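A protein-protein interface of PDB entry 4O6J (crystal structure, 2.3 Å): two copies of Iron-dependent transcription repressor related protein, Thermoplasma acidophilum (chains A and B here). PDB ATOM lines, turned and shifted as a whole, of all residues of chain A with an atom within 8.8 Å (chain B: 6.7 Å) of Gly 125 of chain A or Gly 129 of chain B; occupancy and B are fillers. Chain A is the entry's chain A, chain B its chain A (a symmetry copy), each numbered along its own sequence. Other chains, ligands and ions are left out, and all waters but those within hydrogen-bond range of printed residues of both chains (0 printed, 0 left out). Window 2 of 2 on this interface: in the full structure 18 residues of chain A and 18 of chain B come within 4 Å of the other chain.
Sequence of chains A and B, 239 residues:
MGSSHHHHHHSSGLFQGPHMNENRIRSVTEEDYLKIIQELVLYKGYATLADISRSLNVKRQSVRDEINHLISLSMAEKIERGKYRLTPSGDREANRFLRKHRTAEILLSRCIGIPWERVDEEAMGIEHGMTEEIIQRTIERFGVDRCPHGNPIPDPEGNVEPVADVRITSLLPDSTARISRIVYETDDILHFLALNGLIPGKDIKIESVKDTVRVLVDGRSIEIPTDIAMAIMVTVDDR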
ATOM      1  N   ARG A  26      12.436   9.337  -2.649  1.00  0.00           N
ATOM      2  CA  ARG A  26      12.023  10.101  -1.474  1.00  0.00           C
ATOM      3  C   ARG A  26      10.962  11.144  -1.838  1.00  0.00           C
ATOM      4  O   ARG A  26      11.057  11.787  -2.883  1.00  0.00           O
ATOM      5  CB  ARG A  26      13.234  10.775  -0.827  1.00  0.00           C
ATOM      6  N   SER A  27       9.944  11.300  -0.990  1.00  0.00           N
ATOM      7  CA  SER A  27       9.017  12.417  -1.144  1.00  0.00           C
ATOM      8  C   SER A  27       9.622  13.650  -0.473  1.00  0.00           C
ATOM      9  O   SER A  27      10.641  13.559   0.215  1.00  0.00           O
ATOM     10  CB  SER A  27       7.646  12.113  -0.548  1.00  0.00           C
ATOM     11  OG  SER A  27       7.641  12.377   0.843  1.00  0.00           O
ATOM     12  N   ASP A  32      14.519  19.592   2.120  1.00  0.00           N
ATOM     13  CA  ASP A  32      14.615  19.863   0.688  1.00  0.00           C
ATOM     14  C   ASP A  32      14.253  21.316   0.372  1.00  0.00           C
ATOM     15  O   ASP A  32      14.822  21.918  -0.527  1.00  0.00           O
ATOM     16  CB  ASP A  32      13.704  18.932  -0.105  1.00  0.00           C
ATOM     17  CG  ASP A  32      14.025  17.479   0.133  1.00  0.00           C
ATOM     18  OD1 ASP A  32      15.187  17.073  -0.102  1.00  0.00           O
ATOM     19  OD2 ASP A  32      13.123  16.752   0.585  1.00  0.00           O
ATOM     20  N   PHE A  97      21.688  20.143   7.443  1.00  0.00           N
ATOM     21  CA  PHE A  97      21.251  19.160   6.473  1.00  0.00           C
ATOM     22  C   PHE A  97      22.323  18.954   5.400  1.00  0.00           C
ATOM     23  O   PHE A  97      22.593  17.834   4.992  1.00  0.00           O
ATOM     24  CB  PHE A  97      19.932  19.572   5.819  1.00  0.00           C
ATOM     25  CG  PHE A  97      19.516  18.677   4.672  1.00  0.00           C
ATOM     26  CD1 PHE A  97      19.186  17.343   4.895  1.00  0.00           C
ATOM     27  CD2 PHE A  97      19.446  19.171   3.375  1.00  0.00           C
ATOM     28  CE1 PHE A  97      18.795  16.514   3.838  1.00  0.00           C
ATOM     29  CE2 PHE A  97      19.058  18.359   2.314  1.00  0.00           C
ATOM     30  CZ  PHE A  97      18.729  17.033   2.541  1.00  0.00           C
ATOM     31  N   HIS A 101      23.964  15.910   3.260  1.00  0.00           N
ATOM     32  CA  HIS A 101      23.887  15.834   1.816  1.00  0.00           C
ATOM     33  C   HIS A 101      25.274  15.719   1.171  1.00  0.00           C
ATOM     34  O   HIS A 101      25.528  14.838   0.346  1.00  0.00           O
ATOM     35  CB  HIS A 101      23.158  17.065   1.270  1.00  0.00           C
ATOM     36  CG  HIS A 101      23.253  17.202  -0.211  1.00  0.00           C
ATOM     37  ND1 HIS A 101      22.609  16.345  -1.078  1.00  0.00           N
ATOM     38  CD2 HIS A 101      23.940  18.074  -0.984  1.00  0.00           C
ATOM     39  CE1 HIS A 101      22.882  16.692  -2.320  1.00  0.00           C
ATOM     40  NE2 HIS A 101      23.686  17.740  -2.291  1.00  0.00           N
ATOM     41  N   ALA A 104      27.180  12.632   1.812  1.00  0.00           N
ATOM     42  CA  ALA A 104      26.567  11.526   1.093  1.00  0.00           C
ATOM     43  C   ALA A 104      27.104  11.525  -0.328  1.00  0.00           C
ATOM     44  O   ALA A 104      27.420  10.483  -0.867  1.00  0.00           O
ATOM     45  CB  ALA A 104      25.056  11.645   1.092  1.00  0.00           C
ATOM     46  N   LEU A 108      29.062   8.508  -2.099  1.00  0.00           N
ATOM     47  CA  LEU A 108      28.594   7.879  -3.329  1.00  0.00           C
ATOM     48  C   LEU A 108      29.581   7.992  -4.489  1.00  0.00           C
ATOM     49  O   LEU A 108      29.729   7.054  -5.272  1.00  0.00           O
ATOM     50  CB  LEU A 108      27.253   8.476  -3.738  1.00  0.00           C
ATOM     51  CG  LEU A 108      26.112   8.146  -2.785  1.00  0.00           C
ATOM     52  CD1 LEU A 108      24.804   8.694  -3.347  1.00  0.00           C
ATOM     53  CD2 LEU A 108      26.033   6.596  -2.594  1.00  0.00           C
ATOM     54  N   VAL A 119      25.508  12.813  -8.932  1.00  0.00           N
ATOM     55  CA  VAL A 119      25.637  12.432  -7.534  1.00  0.00           C
ATOM     56  C   VAL A 119      24.821  13.355  -6.621  1.00  0.00           C
ATOM     57  O   VAL A 119      24.536  13.013  -5.476  1.00  0.00           O
ATOM     58  CB  VAL A 119      27.141  12.403  -7.101  1.00  0.00           C
ATOM     59  CG1 VAL A 119      27.675  13.810  -6.839  1.00  0.00           C
ATOM     60  CG2 VAL A 119      27.336  11.507  -5.887  1.00  0.00           C
ATOM     61  N   ASP A 120      24.413  14.505  -7.139  1.00  0.00           N
ATOM     62  CA  ASP A 120      23.541  15.403  -6.380  1.00  0.00           C
ATOM     63  C   ASP A 120      22.141  14.778  -6.288  1.00  0.00           C
ATOM     64  O   ASP A 120      21.545  14.718  -5.220  1.00  0.00           O
ATOM     65  CB  ASP A 120      23.493  16.801  -7.024  1.00  0.00           C
ATOM     66  CG  ASP A 120      22.492  17.743  -6.341  1.00  0.00           C
ATOM     67  OD1 ASP A 120      22.696  18.094  -5.160  1.00  0.00           O
ATOM     68  OD2 ASP A 120      21.504  18.146  -6.992  1.00  0.00           O
ATOM     69  N   GLU A 121      21.640  14.270  -7.405  1.00  0.00           N
ATOM     70  CA  GLU A 121      20.351  13.571  -7.409  1.00  0.00           C
ATOM     71  C   GLU A 121      20.375  12.277  -6.569  1.00  0.00           C
ATOM     72  O   GLU A 121      19.474  12.028  -5.790  1.00  0.00           O
ATOM     73  CB  GLU A 121      19.930  13.227  -8.843  1.00  0.00           C
ATOM     74  CG  GLU A 121      19.779  14.400  -9.778  1.00  0.00           C
ATOM     75  CD  GLU A 121      18.519  15.197  -9.500  1.00  0.00           C
ATOM     76  OE1 GLU A 121      17.527  14.582  -9.046  1.00  0.00           O
ATOM     77  OE2 GLU A 121      18.525  16.430  -9.733  1.00  0.00           O
ATOM     78  N   GLU A 122      21.392  11.438  -6.755  1.00  0.00           N
ATOM     79  CA  GLU A 122      21.439  10.139  -6.078  1.00  0.00           C
ATOM     80  C   GLU A 122      21.660  10.230  -4.567  1.00  0.00           C
ATOM     81  O   GLU A 122      21.408   9.270  -3.857  1.00  0.00           O
ATOM     82  CB  GLU A 122      22.541   9.251  -6.672  1.00  0.00           C
ATOM     83  CG  GLU A 122      22.318   8.786  -8.107  1.00  0.00           C
ATOM     84  CD  GLU A 122      21.099   7.902  -8.277  1.00  0.00           C
ATOM     85  OE1 GLU A 122      20.715   7.201  -7.315  1.00  0.00           O
ATOM     86  OE2 GLU A 122      20.528   7.907  -9.390  1.00  0.00           O
ATOM     87  N   ALA A 123      22.158  11.358  -4.067  1.00  0.00           N
ATOM     88  CA  ALA A 123      22.370  11.471  -2.632  1.00  0.00           C
ATOM     89  C   ALA A 123      21.041  11.670  -1.922  1.00  0.00           C
ATOM     90  O   ALA A 123      20.946  11.531  -0.710  1.00  0.00           O
ATOM     91  CB  ALA A 123      23.343  12.633  -2.310  1.00  0.00           C
ATOM     92  N   MET A 124      20.016  11.996  -2.695  1.00  0.00           N
ATOM     93  CA  MET A 124      18.703  12.327  -2.164  1.00  0.00           C
ATOM     94  C   MET A 124      18.084  11.244  -1.290  1.00  0.00           C
ATOM     95  O   MET A 124      17.431  11.544  -0.292  1.00  0.00           O
ATOM     96  CB  MET A 124      17.755  12.638  -3.311  1.00  0.00           C
ATOM     97  CG  MET A 124      17.347  14.092  -3.332  1.00  0.00           C
ATOM     98  SD  MET A 124      15.986  14.369  -4.456  1.00  0.00           S
ATOM     99  CE  MET A 124      14.723  13.428  -3.600  1.00  0.00           C
ATOM    100  N   GLY A 125      18.284   9.993  -1.674  1.00  0.00           N
ATOM    101  CA  GLY A 125      17.778   8.879  -0.899  1.00  0.00           C
ATOM    102  C   GLY A 125      18.459   8.746   0.451  1.00  0.00           C
ATOM    103  O   GLY A 125      17.800   8.834   1.489  1.00  0.00           O
ATOM    104  N   ILE A 126      19.780   8.565   0.445  1.00  0.00           N
ATOM    105  CA  ILE A 126      20.478   8.175   1.661  1.00  0.00           C
ATOM    106  C   ILE A 126      20.812   9.313   2.620  1.00  0.00           C
ATOM    107  O   ILE A 126      21.214   9.066   3.757  1.00  0.00           O
ATOM    108  CB  ILE A 126      21.771   7.449   1.335  1.00  0.00           C
ATOM    109  CG1 ILE A 126      22.755   8.381   0.668  1.00  0.00           C
ATOM    110  CG2 ILE A 126      21.477   6.242   0.424  1.00  0.00           C
ATOM    111  CD1 ILE A 126      24.221   7.881   0.730  1.00  0.00           C
ATOM    112  N   GLU A 127      20.648  10.553   2.192  1.00  0.00           N
ATOM    113  CA  GLU A 127      21.142  11.655   3.001  1.00  0.00           C
ATOM    114  C   GLU A 127      20.370  11.833   4.320  1.00  0.00           C
ATOM    115  O   GLU A 127      20.969  12.114   5.360  1.00  0.00           O
ATOM    116  CB  GLU A 127      21.132  12.956   2.193  1.00  0.00           C
ATOM    117  CG  GLU A 127      19.788  13.384   1.644  1.00  0.00           C
ATOM    118  CD  GLU A 127      19.917  14.347   0.448  1.00  0.00           C
ATOM    119  OE1 GLU A 127      21.034  14.507  -0.116  1.00  0.00           O
ATOM    120  OE2 GLU A 127      18.890  14.951   0.069  1.00  0.00           O
ATOM    121  N   HIS A 128      19.057  11.647   4.300  1.00  0.00           N
ATOM    122  CA  HIS A 128      18.272  11.909   5.512  1.00  0.00           C
ATOM    123  C   HIS A 128      18.722  11.115   6.728  1.00  0.00           C
ATOM    124  O   HIS A 128      18.612  11.589   7.844  1.00  0.00           O
ATOM    125  CB  HIS A 128      16.794  11.648   5.256  1.00  0.00           C
ATOM    126  CG  HIS A 128      16.084  12.831   4.693  1.00  0.00           C
ATOM    127  ND1 HIS A 128      16.254  13.246   3.389  1.00  0.00           N
ATOM    128  CD2 HIS A 128      15.243  13.720   5.266  1.00  0.00           C
ATOM    129  CE1 HIS A 128      15.532  14.332   3.178  1.00  0.00           C
ATOM    130  NE2 HIS A 128      14.909  14.641   4.302  1.00  0.00           N
ATOM    131  N   GLY A 129      19.251   9.919   6.506  1.00  0.00           N
ATOM    132  CA  GLY A 129      19.663   9.056   7.599  1.00  0.00           C
ATOM    133  C   GLY A 129      21.158   9.010   7.877  1.00  0.00           C
ATOM    134  O   GLY A 129      21.602   8.177   8.659  1.00  0.00           O
ATOM    135  N   MET A 130      21.937   9.886   7.237  1.00  0.00           N
ATOM    136  CA  MET A 130      23.367   9.997   7.538  1.00  0.00           C
ATOM    137  C   MET A 130      23.571  10.414   9.009  1.00  0.00           C
ATOM    138  O   MET A 130      23.218  11.520   9.402  1.00  0.00           O
ATOM    139  CB  MET A 130      24.052  11.007   6.603  1.00  0.00           C
ATOM    140  CG  MET A 130      23.960  10.697   5.117  1.00  0.00           C
ATOM    141  SD  MET A 130      25.192   9.465   4.573  1.00  0.00           S
ATOM    142  CE  MET A 130      26.705  10.313   5.003  1.00  0.00           C
ATOM    143  N   LYS B 100      17.951  -3.607   0.157  1.00  0.00           N
ATOM    144  CA  LYS B 100      18.430  -2.279   0.541  1.00  0.00           C
ATOM    145  C   LYS B 100      19.285  -2.340   1.791  1.00  0.00           C
ATOM    146  O   LYS B 100      20.375  -1.786   1.840  1.00  0.00           O
ATOM    147  CB  LYS B 100      17.255  -1.340   0.783  1.00  0.00           C
ATOM    148  CG  LYS B 100      16.350  -1.116  -0.442  1.00  0.00           C
ATOM    149  CD  LYS B 100      15.228  -0.119  -0.054  1.00  0.00           C
ATOM    150  CE  LYS B 100      14.329   0.265  -1.216  1.00  0.00           C
ATOM    151  NZ  LYS B 100      13.366  -0.812  -1.572  1.00  0.00           N
ATOM    152  N   GLY B 125      19.814   4.149   9.081  1.00  0.00           N
ATOM    153  CA  GLY B 125      19.573   5.462   8.521  1.00  0.00           C
ATOM    154  C   GLY B 125      19.461   5.443   7.007  1.00  0.00           C
ATOM    155  O   GLY B 125      18.419   5.810   6.458  1.00  0.00           O
ATOM    156  N   ILE B 126      20.516   4.988   6.330  1.00  0.00           N
ATOM    157  CA  ILE B 126      20.601   5.168   4.888  1.00  0.00           C
ATOM    158  C   ILE B 126      19.841   4.144   4.051  1.00  0.00           C
ATOM    159  O   ILE B 126      19.683   4.326   2.845  1.00  0.00           O
ATOM    160  CB  ILE B 126      22.048   5.161   4.426  1.00  0.00           C
ATOM    161  CG1 ILE B 126      22.669   3.800   4.632  1.00  0.00           C
ATOM    162  CG2 ILE B 126      22.847   6.233   5.192  1.00  0.00           C
ATOM    163  CD1 ILE B 126      23.944   3.566   3.782  1.00  0.00           C
ATOM    164  N   GLU B 127      19.359   3.077   4.666  1.00  0.00           N
ATOM    165  CA  GLU B 127      18.807   1.991   3.873  1.00  0.00           C
ATOM    166  C   GLU B 127      17.502   2.369   3.152  1.00  0.00           C
ATOM    167  O   GLU B 127      17.292   1.983   2.000  1.00  0.00           O
ATOM    168  CB  GLU B 127      18.599   0.748   4.744  1.00  0.00           C
ATOM    169  CG  GLU B 127      17.690   0.924   5.941  1.00  0.00           C
ATOM    170  CD  GLU B 127      17.934  -0.140   7.030  1.00  0.00           C
ATOM    171  OE1 GLU B 127      18.959  -0.873   6.978  1.00  0.00           O
ATOM    172  OE2 GLU B 127      17.089  -0.243   7.947  1.00  0.00           O
ATOM    173  N   HIS B 128      16.636   3.138   3.799  1.00  0.00           N
ATOM    174  CA  HIS B 128      15.335   3.434   3.186  1.00  0.00           C
ATOM    175  C   HIS B 128      15.427   4.083   1.814  1.00  0.00           C
ATOM    176  O   HIS B 128      14.571   3.867   0.976  1.00  0.00           O
ATOM    177  CB  HIS B 128      14.501   4.314   4.108  1.00  0.00           C
ATOM    178  CG  HIS B 128      13.713   3.531   5.102  1.00  0.00           C
ATOM    179  ND1 HIS B 128      14.295   2.915   6.189  1.00  0.00           N
ATOM    180  CD2 HIS B 128      12.399   3.219   5.148  1.00  0.00           C
ATOM    181  CE1 HIS B 128      13.368   2.271   6.874  1.00  0.00           C
ATOM    182  NE2 HIS B 128      12.207   2.439   6.263  1.00  0.00           N
ATOM    183  N   GLY B 129      16.480   4.855   1.582  1.00  0.00           N
ATOM    184  CA  GLY B 129      16.636   5.566   0.325  1.00  0.00           C
ATOM    185  C   GLY B 129      17.615   4.950  -0.664  1.00  0.00           C
ATOM    186  O   GLY B 129      17.936   5.579  -1.667  1.00  0.00           O
ATOM    187  N   MET B 130      18.098   3.737  -0.387  1.00  0.00           N
ATOM    188  CA  MET B 130      18.945   3.016  -1.343  1.00  0.00           C
ATOM    189  C   MET B 130      18.168   2.753  -2.649  1.00  0.00           C
ATOM    190  O   MET B 130      17.200   2.000  -2.662  1.00  0.00           O
ATOM    191  CB  MET B 130      19.444   1.689  -0.748  1.00  0.00           C
ATOM    192  CG  MET B 130      20.261   1.805   0.529  1.00  0.00           C
ATOM    193  SD  MET B 130      22.006   2.241   0.217  1.00  0.00           S
ATOM    194  CE  MET B 130      22.507   0.854  -0.793  1.00  0.00           C
ATOM    195  N   THR B 131      18.573   3.413  -3.729  1.00  0.00           N
ATOM    196  CA  THR B 131      17.972   3.217  -5.042  1.00  0.00           C
ATOM    197  C   THR B 131      18.620   2.032  -5.749  1.00  0.00           C
ATOM    198  O   THR B 131      19.698   1.594  -5.353  1.00  0.00           O
ATOM    199  CB  THR B 131      18.159   4.423  -5.924  1.00  0.00           C
ATOM    200  OG1 THR B 131      19.563   4.629  -6.116  1.00  0.00           O
ATOM    201  CG2 THR B 131      17.527   5.677  -5.291  1.00  0.00           C
ATOM    202  N   GLU B 132      17.984   1.535  -6.809  1.00  0.00           N
ATOM    203  CA  GLU B 132      18.591   0.493  -7.631  1.00  0.00           C
ATOM    204  C   GLU B 132      19.916   0.938  -8.249  1.00  0.00           C
ATOM    205  O   GLU B 132      20.816   0.123  -8.432  1.00  0.00           O
ATOM    206  CB  GLU B 132      17.623   0.046  -8.733  1.00  0.00           C
ATOM    207  CG  GLU B 132      16.664  -1.061  -8.273  1.00  0.00           C
ATOM    208  CD  GLU B 132      17.389  -2.234  -7.591  1.00  0.00           C
ATOM    209  OE1 GLU B 132      18.384  -2.759  -8.162  1.00  0.00           O
ATOM    210  OE2 GLU B 132      16.970  -2.613  -6.472  1.00  0.00           O
ATOM    211  N   ILE B 134      22.166   2.906  -6.815  1.00  0.00           N
ATOM    212  CA  ILE B 134      23.163   2.753  -5.755  1.00  0.00           C
ATOM    213  C   ILE B 134      23.404   1.268  -5.440  1.00  0.00           C
ATOM    214  O   ILE B 134      24.547   0.824  -5.347  1.00  0.00           O
ATOM    215  CB  ILE B 134      22.728   3.492  -4.473  1.00  0.00           C
ATOM    216  CG1 ILE B 134      22.700   5.009  -4.728  1.00  0.00           C
ATOM    217  CG2 ILE B 134      23.666   3.144  -3.311  1.00  0.00           C
ATOM    218  CD1 ILE B 134      22.147   5.829  -3.550  1.00  0.00           C
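Gly 125 of chain A touches just one residue of chain B: Gly 129 (3.4 Å).
Of the printed residues of chain B, Ile 126 of chain A touches Ile 126 (3.6 Å).
Of the printed residues of chain B, Gly 129 of chain A touches Gly 125.
Printed residues of chain A within 4 Å of Gly 125 of chain B: Gly 129.
Met 130 of chain B touches none of the printed residues of chain A.
Printed residues of chain A within 4 Å of Ile 134 of chain B: Leu 108 (3.9 Å) and Glu 122 (3.5 Å).
The nearest residue of chain A that does not touch Gly 129 of chain B is Ile 126 of chain A (4.1 Å).
The side-chain hydroxyl (OG1) of Thr 131 of chain B is in hydrogen-bond range of the side-chain carboxylate (OE1) of Glu 122 of chain A, 3.1 Å away.
Gly 125 of chain A touches Gly 129 of chain B, and with the chains exchanged Gly 129 of chain A touches Gly 125 of chain B.
Ile 126 of chain A touches its own counterpart, Ile 126 of chain B.
Of the 6 pairs that touch across the chains among the printed residues, 3 have their exchanged pair printed and touching as well.
Of the 10 printed residues of chain B, 5 touch a printed residue of chain A.
Hydrophobic or aromatic side chains of chain A that line the printed part of chain B: Leu 108 and Ile 126.
Among the printed residues, 6 pairs touch across the chains.
Among the printed residues, no Asp or Glu carboxylate lies within 4 Å of a Lys or Arg side-chain nitrogen of the other chain.
N of Ile 134 of chain B lies within hydrogen-bond range of OG1 of Thr 131 of chain B, at 3.2 Å.
CD1 of Leu 108 of chain A touches CD1 of Ile 134 of chain B, 3.9 Å away.
Ile 134 of chain B touches Glu 122 of chain A.
Gly 129 of chain B touches Gly 125 of chain A (O to CA, 3.4 Å).
CG2 of Ile 126 of chain A touches O of Ile 126 of chain B (3.6 Å).
Gly 129 of chain A touches Gly 125 of chain B (O to CA, 3.4 Å).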
